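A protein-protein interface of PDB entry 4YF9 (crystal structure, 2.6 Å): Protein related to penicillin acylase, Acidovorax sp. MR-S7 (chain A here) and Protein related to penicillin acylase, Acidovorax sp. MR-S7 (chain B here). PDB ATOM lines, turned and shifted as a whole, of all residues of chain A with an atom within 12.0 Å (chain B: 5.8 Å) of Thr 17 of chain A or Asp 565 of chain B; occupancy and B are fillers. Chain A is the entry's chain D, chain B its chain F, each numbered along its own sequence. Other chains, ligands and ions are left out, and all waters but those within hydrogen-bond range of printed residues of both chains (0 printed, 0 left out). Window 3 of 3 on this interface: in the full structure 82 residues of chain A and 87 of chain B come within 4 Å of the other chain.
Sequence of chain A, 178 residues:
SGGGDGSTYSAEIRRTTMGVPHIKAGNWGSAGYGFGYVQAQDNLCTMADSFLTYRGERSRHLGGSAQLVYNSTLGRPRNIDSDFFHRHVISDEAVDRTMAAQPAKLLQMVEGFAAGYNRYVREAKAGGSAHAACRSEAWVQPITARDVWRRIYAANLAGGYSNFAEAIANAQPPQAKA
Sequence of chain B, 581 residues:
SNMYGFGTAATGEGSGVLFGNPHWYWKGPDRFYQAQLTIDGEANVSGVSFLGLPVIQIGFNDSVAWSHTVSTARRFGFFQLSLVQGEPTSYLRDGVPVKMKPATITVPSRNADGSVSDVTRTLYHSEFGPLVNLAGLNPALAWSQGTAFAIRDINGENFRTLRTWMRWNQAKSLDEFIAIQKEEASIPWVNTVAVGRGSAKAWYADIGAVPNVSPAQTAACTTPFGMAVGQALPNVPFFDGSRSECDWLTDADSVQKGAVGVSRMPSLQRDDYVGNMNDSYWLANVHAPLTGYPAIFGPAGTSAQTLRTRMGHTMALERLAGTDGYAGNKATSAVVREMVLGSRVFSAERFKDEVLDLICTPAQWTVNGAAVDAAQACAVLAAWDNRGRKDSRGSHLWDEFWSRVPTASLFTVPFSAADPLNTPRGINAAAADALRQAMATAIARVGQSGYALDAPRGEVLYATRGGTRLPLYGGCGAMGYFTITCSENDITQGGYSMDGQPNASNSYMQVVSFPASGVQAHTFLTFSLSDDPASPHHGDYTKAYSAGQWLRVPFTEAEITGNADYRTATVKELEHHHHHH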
ATOM      1  N   GLU A  12     -23.014 -22.045  14.750  1.00  0.00           N
ATOM      2  CA  GLU A  12     -21.982 -21.749  15.727  1.00  0.00           C
ATOM      3  C   GLU A  12     -22.284 -20.371  16.319  1.00  0.00           C
ATOM      4  O   GLU A  12     -22.538 -19.402  15.592  1.00  0.00           O
ATOM      5  CB  GLU A  12     -20.589 -21.796  15.102  1.00  0.00           C
ATOM      6  CG  GLU A  12     -19.475 -21.823  16.136  1.00  0.00           C
ATOM      7  CD  GLU A  12     -18.096 -21.599  15.537  1.00  0.00           C
ATOM      8  OE1 GLU A  12     -17.958 -21.666  14.287  1.00  0.00           O
ATOM      9  OE2 GLU A  12     -17.146 -21.359  16.318  1.00  0.00           O
ATOM     10  N   ILE A  13     -22.283 -20.312  17.644  1.00  0.00           N
ATOM     11  CA  ILE A  13     -22.610 -19.117  18.390  1.00  0.00           C
ATOM     12  C   ILE A  13     -21.343 -18.639  19.072  1.00  0.00           C
ATOM     13  O   ILE A  13     -20.821 -19.316  19.948  1.00  0.00           O
ATOM     14  CB  ILE A  13     -23.684 -19.404  19.468  1.00  0.00           C
ATOM     15  CG1 ILE A  13     -24.913 -20.062  18.832  1.00  0.00           C
ATOM     16  CG2 ILE A  13     -24.055 -18.126  20.206  1.00  0.00           C
ATOM     17  CD1 ILE A  13     -26.013 -20.398  19.813  1.00  0.00           C
ATOM     18  N   ARG A  14     -20.839 -17.485  18.652  1.00  0.00           N
ATOM     19  CA  ARG A  14     -19.646 -16.917  19.264  1.00  0.00           C
ATOM     20  C   ARG A  14     -20.059 -15.677  20.020  1.00  0.00           C
ATOM     21  O   ARG A  14     -20.639 -14.758  19.435  1.00  0.00           O
ATOM     22  CB  ARG A  14     -18.588 -16.557  18.216  1.00  0.00           C
ATOM     23  CG  ARG A  14     -18.009 -17.733  17.447  1.00  0.00           C
ATOM     24  CD  ARG A  14     -18.875 -18.084  16.248  1.00  0.00           C
ATOM     25  NE  ARG A  14     -19.052 -16.935  15.352  1.00  0.00           N
ATOM     26  CZ  ARG A  14     -18.224 -16.631  14.353  1.00  0.00           C
ATOM     27  NH1 ARG A  14     -17.163 -17.386  14.121  1.00  0.00           N
ATOM     28  NH2 ARG A  14     -18.453 -15.569  13.587  1.00  0.00           N
ATOM     29  N   ARG A  15     -19.786 -15.668  21.322  1.00  0.00           N
ATOM     30  CA  ARG A  15     -20.095 -14.515  22.159  1.00  0.00           C
ATOM     31  C   ARG A  15     -18.823 -13.776  22.527  1.00  0.00           C
ATOM     32  O   ARG A  15     -17.768 -14.392  22.725  1.00  0.00           O
ATOM     33  CB  ARG A  15     -20.868 -14.921  23.418  1.00  0.00           C
ATOM     34  CG  ARG A  15     -22.300 -15.336  23.124  1.00  0.00           C
ATOM     35  CD  ARG A  15     -23.176 -15.243  24.351  1.00  0.00           C
ATOM     36  NE  ARG A  15     -24.519 -15.773  24.110  1.00  0.00           N
ATOM     37  CZ  ARG A  15     -25.631 -15.042  24.074  1.00  0.00           C
ATOM     38  NH1 ARG A  15     -26.805 -15.632  23.864  1.00  0.00           N
ATOM     39  NH2 ARG A  15     -25.573 -13.726  24.251  1.00  0.00           N
ATOM     40  N   THR A  16     -18.927 -12.451  22.580  1.00  0.00           N
ATOM     41  CA  THR A  16     -17.811 -11.593  22.956  1.00  0.00           C
ATOM     42  C   THR A  16     -18.241 -10.667  24.088  1.00  0.00           C
ATOM     43  O   THR A  16     -19.328 -10.828  24.640  1.00  0.00           O
ATOM     44  CB  THR A  16     -17.343 -10.747  21.772  1.00  0.00           C
ATOM     45  OG1 THR A  16     -18.414  -9.891  21.350  1.00  0.00           O
ATOM     46  CG2 THR A  16     -16.907 -11.638  20.616  1.00  0.00           C
ATOM     47  N   THR A  17     -17.387  -9.704  24.423  1.00  0.00           N
ATOM     48  CA  THR A  17     -17.713  -8.656  25.387  1.00  0.00           C
ATOM     49  C   THR A  17     -19.157  -8.146  25.264  1.00  0.00           C
ATOM     50  O   THR A  17     -19.666  -7.943  24.160  1.00  0.00           O
ATOM     51  CB  THR A  17     -16.747  -7.476  25.256  1.00  0.00           C
ATOM     52  OG1 THR A  17     -15.419  -7.988  25.143  1.00  0.00           O
ATOM     53  CG2 THR A  17     -16.826  -6.571  26.486  1.00  0.00           C
ATOM     54  N   MET A  18     -19.790  -7.954  26.424  1.00  0.00           N
ATOM     55  CA  MET A  18     -21.208  -7.603  26.549  1.00  0.00           C
ATOM     56  C   MET A  18     -22.169  -8.716  26.119  1.00  0.00           C
ATOM     57  O   MET A  18     -23.381  -8.506  26.077  1.00  0.00           O
ATOM     58  CB  MET A  18     -21.538  -6.278  25.841  1.00  0.00           C
ATOM     59  CG  MET A  18     -20.548  -5.158  26.126  1.00  0.00           C
ATOM     60  SD  MET A  18     -20.275  -4.802  27.872  1.00  0.00           S
ATOM     61  CE  MET A  18     -18.986  -3.559  27.742  1.00  0.00           C
ATOM     62  N   GLY A  19     -21.624  -9.896  25.827  1.00  0.00           N
ATOM     63  CA  GLY A  19     -22.422 -11.061  25.435  1.00  0.00           C
ATOM     64  C   GLY A  19     -22.890 -11.047  23.988  1.00  0.00           C
ATOM     65  O   GLY A  19     -23.628 -11.946  23.568  1.00  0.00           O
ATOM     66  N   VAL A  20     -22.467 -10.029  23.234  1.00  0.00           N
ATOM     67  CA  VAL A  20     -22.822  -9.886  21.827  1.00  0.00           C
ATOM     68  C   VAL A  20     -22.571 -11.190  21.059  1.00  0.00           C
ATOM     69  O   VAL A  20     -21.421 -11.623  20.920  1.00  0.00           O
ATOM     70  CB  VAL A  20     -22.077  -8.703  21.152  1.00  0.00           C
ATOM     71  CG1 VAL A  20     -22.470  -8.589  19.686  1.00  0.00           C
ATOM     72  CG2 VAL A  20     -22.377  -7.389  21.864  1.00  0.00           C
ATOM     73  N   PRO A  21     -23.657 -11.836  20.585  1.00  0.00           N
ATOM     74  CA  PRO A  21     -23.545 -13.100  19.856  1.00  0.00           C
ATOM     75  C   PRO A  21     -23.283 -12.873  18.377  1.00  0.00           C
ATOM     76  O   PRO A  21     -23.889 -11.979  17.773  1.00  0.00           O
ATOM     77  CB  PRO A  21     -24.916 -13.733  20.052  1.00  0.00           C
ATOM     78  CG  PRO A  21     -25.848 -12.565  20.192  1.00  0.00           C
ATOM     79  CD  PRO A  21     -25.061 -11.420  20.761  1.00  0.00           C
ATOM     80  N   HIS A  22     -22.371 -13.669  17.814  1.00  0.00           N
ATOM     81  CA  HIS A  22     -22.069 -13.663  16.380  1.00  0.00           C
ATOM     82  C   HIS A  22     -22.380 -15.031  15.828  1.00  0.00           C
ATOM     83  O   HIS A  22     -21.600 -15.960  16.000  1.00  0.00           O
ATOM     84  CB  HIS A  22     -20.593 -13.314  16.139  1.00  0.00           C
ATOM     85  CG  HIS A  22     -20.084 -12.147  16.967  1.00  0.00           C
ATOM     86  ND1 HIS A  22     -19.801 -10.942  16.430  1.00  0.00           N
ATOM     87  CD2 HIS A  22     -19.804 -12.042  18.331  1.00  0.00           C
ATOM     88  CE1 HIS A  22     -19.376 -10.107  17.399  1.00  0.00           C
ATOM     89  NE2 HIS A  22     -19.378 -10.782  18.562  1.00  0.00           N
ATOM     90  N   ASP A  42     -31.373 -14.898  26.025  1.00  0.00           N
ATOM     91  CA  ASP A  42     -31.171 -13.646  26.752  1.00  0.00           C
ATOM     92  C   ASP A  42     -32.475 -12.938  27.156  1.00  0.00           C
ATOM     93  O   ASP A  42     -32.481 -12.152  28.116  1.00  0.00           O
ATOM     94  CB  ASP A  42     -30.300 -12.675  25.939  1.00  0.00           C
ATOM     95  CG  ASP A  42     -28.880 -13.179  25.738  1.00  0.00           C
ATOM     96  OD1 ASP A  42     -28.246 -13.592  26.730  1.00  0.00           O
ATOM     97  OD2 ASP A  42     -28.390 -13.154  24.588  1.00  0.00           O
ATOM     98  N   HIS B 537     -25.339 -10.396  31.429  1.00  0.00           N
ATOM     99  CA  HIS B 537     -25.540  -9.342  30.448  1.00  0.00           C
ATOM    100  C   HIS B 537     -26.801  -8.543  30.677  1.00  0.00           C
ATOM    101  O   HIS B 537     -27.410  -8.030  29.723  1.00  0.00           O
ATOM    102  CB  HIS B 537     -25.478  -9.929  29.043  1.00  0.00           C
ATOM    103  CG  HIS B 537     -24.287 -10.833  28.825  1.00  0.00           C
ATOM    104  ND1 HIS B 537     -23.017 -10.397  28.936  1.00  0.00           N
ATOM    105  CD2 HIS B 537     -24.212 -12.191  28.522  1.00  0.00           C
ATOM    106  CE1 HIS B 537     -22.172 -11.419  28.719  1.00  0.00           C
ATOM    107  NE2 HIS B 537     -22.905 -12.515  28.455  1.00  0.00           N
ATOM    108  N   ASP B 540     -23.912  -5.111  32.222  1.00  0.00           N
ATOM    109  CA  ASP B 540     -22.563  -4.780  31.779  1.00  0.00           C
ATOM    110  C   ASP B 540     -22.550  -3.645  30.745  1.00  0.00           C
ATOM    111  O   ASP B 540     -21.856  -2.641  30.929  1.00  0.00           O
ATOM    112  CB  ASP B 540     -21.822  -6.023  31.270  1.00  0.00           C
ATOM    113  CG  ASP B 540     -22.666  -6.890  30.337  1.00  0.00           C
ATOM    114  OD1 ASP B 540     -23.806  -6.501  29.992  1.00  0.00           O
ATOM    115  OD2 ASP B 540     -22.171  -7.978  29.947  1.00  0.00           O
ATOM    116  N   LEU B 551     -18.175   0.482  22.943  1.00  0.00           N
ATOM    117  CA  LEU B 551     -17.708  -0.852  22.615  1.00  0.00           C
ATOM    118  C   LEU B 551     -17.232  -0.919  21.169  1.00  0.00           C
ATOM    119  O   LEU B 551     -17.960  -0.563  20.243  1.00  0.00           O
ATOM    120  CB  LEU B 551     -18.820  -1.880  22.834  1.00  0.00           C
ATOM    121  CG  LEU B 551     -18.381  -3.345  22.726  1.00  0.00           C
ATOM    122  CD1 LEU B 551     -17.548  -3.759  23.929  1.00  0.00           C
ATOM    123  CD2 LEU B 551     -19.604  -4.237  22.554  1.00  0.00           C
ATOM    124  N   ASN B 563     -11.121 -11.664  20.743  1.00  0.00           N
ATOM    125  CA  ASN B 563     -11.751 -10.926  21.829  1.00  0.00           C
ATOM    126  C   ASN B 563     -11.544 -11.577  23.201  1.00  0.00           C
ATOM    127  O   ASN B 563     -11.688 -12.794  23.352  1.00  0.00           O
ATOM    128  CB  ASN B 563     -13.241 -10.756  21.533  1.00  0.00           C
ATOM    129  CG  ASN B 563     -14.006 -10.183  22.705  1.00  0.00           C
ATOM    130  OD1 ASN B 563     -14.509 -10.916  23.538  1.00  0.00           O
ATOM    131  ND2 ASN B 563     -14.086  -8.872  22.776  1.00  0.00           N
ATOM    132  N   ALA B 564     -11.229 -10.749  24.196  1.00  0.00           N
ATOM    133  CA  ALA B 564     -10.917 -11.211  25.553  1.00  0.00           C
ATOM    134  C   ALA B 564     -12.025 -12.063  26.185  1.00  0.00           C
ATOM    135  O   ALA B 564     -11.762 -12.881  27.080  1.00  0.00           O
ATOM    136  CB  ALA B 564     -10.593 -10.026  26.450  1.00  0.00           C
ATOM    137  N   ASP B 565     -13.255 -11.873  25.723  1.00  0.00           N
ATOM    138  CA  ASP B 565     -14.380 -12.609  26.272  1.00  0.00           C
ATOM    139  C   ASP B 565     -14.923 -13.645  25.293  1.00  0.00           C
ATOM    140  O   ASP B 565     -16.095 -14.011  25.359  1.00  0.00           O
ATOM    141  CB  ASP B 565     -15.477 -11.642  26.723  1.00  0.00           C
ATOM    142  CG  ASP B 565     -14.972 -10.623  27.723  1.00  0.00           C
ATOM    143  OD1 ASP B 565     -14.624 -10.998  28.869  1.00  0.00           O
ATOM    144  OD2 ASP B 565     -14.935  -9.435  27.357  1.00  0.00           O
ATOM    145  N   TYR B 566     -14.059 -14.128  24.401  1.00  0.00           N
ATOM    146  CA  TYR B 566     -14.438 -15.120  23.394  1.00  0.00           C
ATOM    147  C   TYR B 566     -14.949 -16.430  23.977  1.00  0.00           C
ATOM    148  O   TYR B 566     -14.236 -17.152  24.667  1.00  0.00           O
ATOM    149  CB  TYR B 566     -13.274 -15.396  22.447  1.00  0.00           C
ATOM    150  CG  TYR B 566     -13.548 -16.445  21.393  1.00  0.00           C
ATOM    151  CD1 TYR B 566     -14.638 -16.331  20.523  1.00  0.00           C
ATOM    152  CD2 TYR B 566     -12.703 -17.534  21.241  1.00  0.00           C
ATOM    153  CE1 TYR B 566     -14.886 -17.287  19.549  1.00  0.00           C
ATOM    154  CE2 TYR B 566     -12.934 -18.489  20.263  1.00  0.00           C
ATOM    155  CZ  TYR B 566     -14.024 -18.366  19.421  1.00  0.00           C
ATOM    156  OH  TYR B 566     -14.257 -19.325  18.461  1.00  0.00           O
ATOM    157  N   ARG B 567     -16.208 -16.712  23.690  1.00  0.00           N
ATOM    158  CA  ARG B 567     -16.801 -17.995  23.987  1.00  0.00           C
ATOM    159  C   ARG B 567     -17.484 -18.500  22.724  1.00  0.00           C
ATOM    160  O   ARG B 567     -18.117 -17.726  21.995  1.00  0.00           O
ATOM    161  CB  ARG B 567     -17.803 -17.866  25.127  1.00  0.00           C
ATOM    162  CG  ARG B 567     -17.179 -17.521  26.475  1.00  0.00           C
ATOM    163  CD  ARG B 567     -16.995 -18.773  27.300  1.00  0.00           C
ATOM    164  NE  ARG B 567     -15.951 -18.687  28.327  1.00  0.00           N
ATOM    165  CZ  ARG B 567     -14.638 -18.773  28.092  1.00  0.00           C
ATOM    166  NH1 ARG B 567     -13.778 -18.727  29.110  1.00  0.00           N
ATOM    167  NH2 ARG B 567     -14.184 -18.906  26.847  1.00  0.00           N
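Of the 12 printed residues of chain A, 7 touch a printed residue of chain B.
Hydrophobic or aromatic side chains of chain A within 4 Å of the printed part of chain B: Met 18.
Among the printed residues, 15 pairs touch across the chains.
The guanidinium group of Arg 15 of chain A is in salt-bridge range of the side-chain carboxylate of Asp 42 of chain A (2.9 Å).
N of Asp 565 of chain B lies within hydrogen-bond range of OD1 of Asn 563 of chain B, at 2.7 Å.
A ring nitrogen (ND1) of His 537 of chain B sits at hydrogen-bond distance from the side-chain carboxylate of Asp 540 of chain B.
The backbone carbonyl oxygen (O) of Gly 19 of chain A sits at hydrogen-bond distance from the guanidinium group (NH2) of Arg 15 of chain A, at 2.7 Å.
The side-chain amide oxygen of Asn 563 of chain B is in hydrogen-bond range of the backbone NH of Tyr 566 of chain B, at 3.4 Å.
The side-chain hydroxyl (OG1) of Thr 16 of chain A is in hydrogen-bond range of the backbone carbonyl oxygen (O) of Val 20 of chain A (3.5 Å).
Of chain B, only Leu 551, Asn 563 and Asp 565 come within 4 Å of Thr 17 of chain A.
Of chain A, only Arg 15 (3.1 Å), Thr 16 (3.8 Å) and Thr 17 (2.7 Å) come within 4 Å of Asp 565 of chain B.
Asn 563 of chain B touches just these residues of chain A: Thr 16 (3.3 Å) and Thr 17 (2.9 Å).
No residue of chain A comes within 4 Å of Ala 564 of chain B.
Arg 567 of chain B touches just these residues of chain A: Ile 13 (3.7 Å), Arg 14 (3.2 Å) and Arg 15 (2.7 Å).
Of the printed residues of chain A, Leu 551 of chain B touches Thr 17 (3.9 Å) and Met 18 (3.8 Å).
Of the printed residues of chain A, His 537 of chain B touches Met 18 (3.4 Å) and Gly 19 (3.3 Å).
Printed residues of chain A within 4 Å of Tyr 566 of chain B: Arg 14 (3.8 Å) and Arg 15 (3.5 Å).
Of the printed residues of chain B, Ile 13 of chain A touches Arg 567.
Of the printed residues of chain B, Thr 16 of chain A touches Asn 563 (3.3 Å) and Asp 565 (3.8 Å).
Glu 12 of chain A touches none of the printed residues of chain B.
The nearest residue of chain A that does not touch Asp 565 of chain B is Met 18 of chain A (5.2 Å).
The nearest printed residue of chain A that does not touch Leu 551 of chain B is Val 20 of chain A (4.3 Å).
The side-chain hydroxyl (OG1) of Thr 17 of chain A sits at hydrogen-bond distance from the side-chain carboxylate (OD2) of Asp 565 of chain B (2.7 Å).
The backbone carbonyl oxygen (O) of Met 18 of chain A sits close to a ring nitrogen (ND1) of His 537 of chain B (3.4 Å).
The backbone carbonyl oxygen (O) of Arg 567 of chain B lies within hydrogen-bond range of the backbone NH (N) of Arg 15 of chain A.
O of Arg 15 of chain A lies close to O of Asp 565 of chain B.
The backbone NH (N) of Gly 19 of chain A sits close to a ring nitrogen (ND1) of His 537 of chain B (3.4 Å).
ND2 of Asn 563 of chain B sits at hydrogen-bond distance from OG1 of Thr 17 of chain A (2.9 Å).
Among the printed residues, merely in contact across the chains: Ile 13 of chain A with Arg 567 of chain B (3.7 Å), Arg 14 of chain A with Tyr 566 of chain B (3.8 Å), Arg 14 of chain A with Arg 567 of chain B (3.2 Å), Arg 15 of chain A with Tyr 566 of chain B (3.5 Å), Thr 16 of chain A with Asn 563 of chain B (3.3 Å), Thr 16 of chain A with Asp 565 of chain B (3.8 Å), Thr 17 of chain A with Leu 551 of chain B (3.9 Å), Met 18 of chain A with Asp 540 of chain B (3.6 Å) and Met 18 of chain A with Leu 551 of chain B (3.8 Å).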
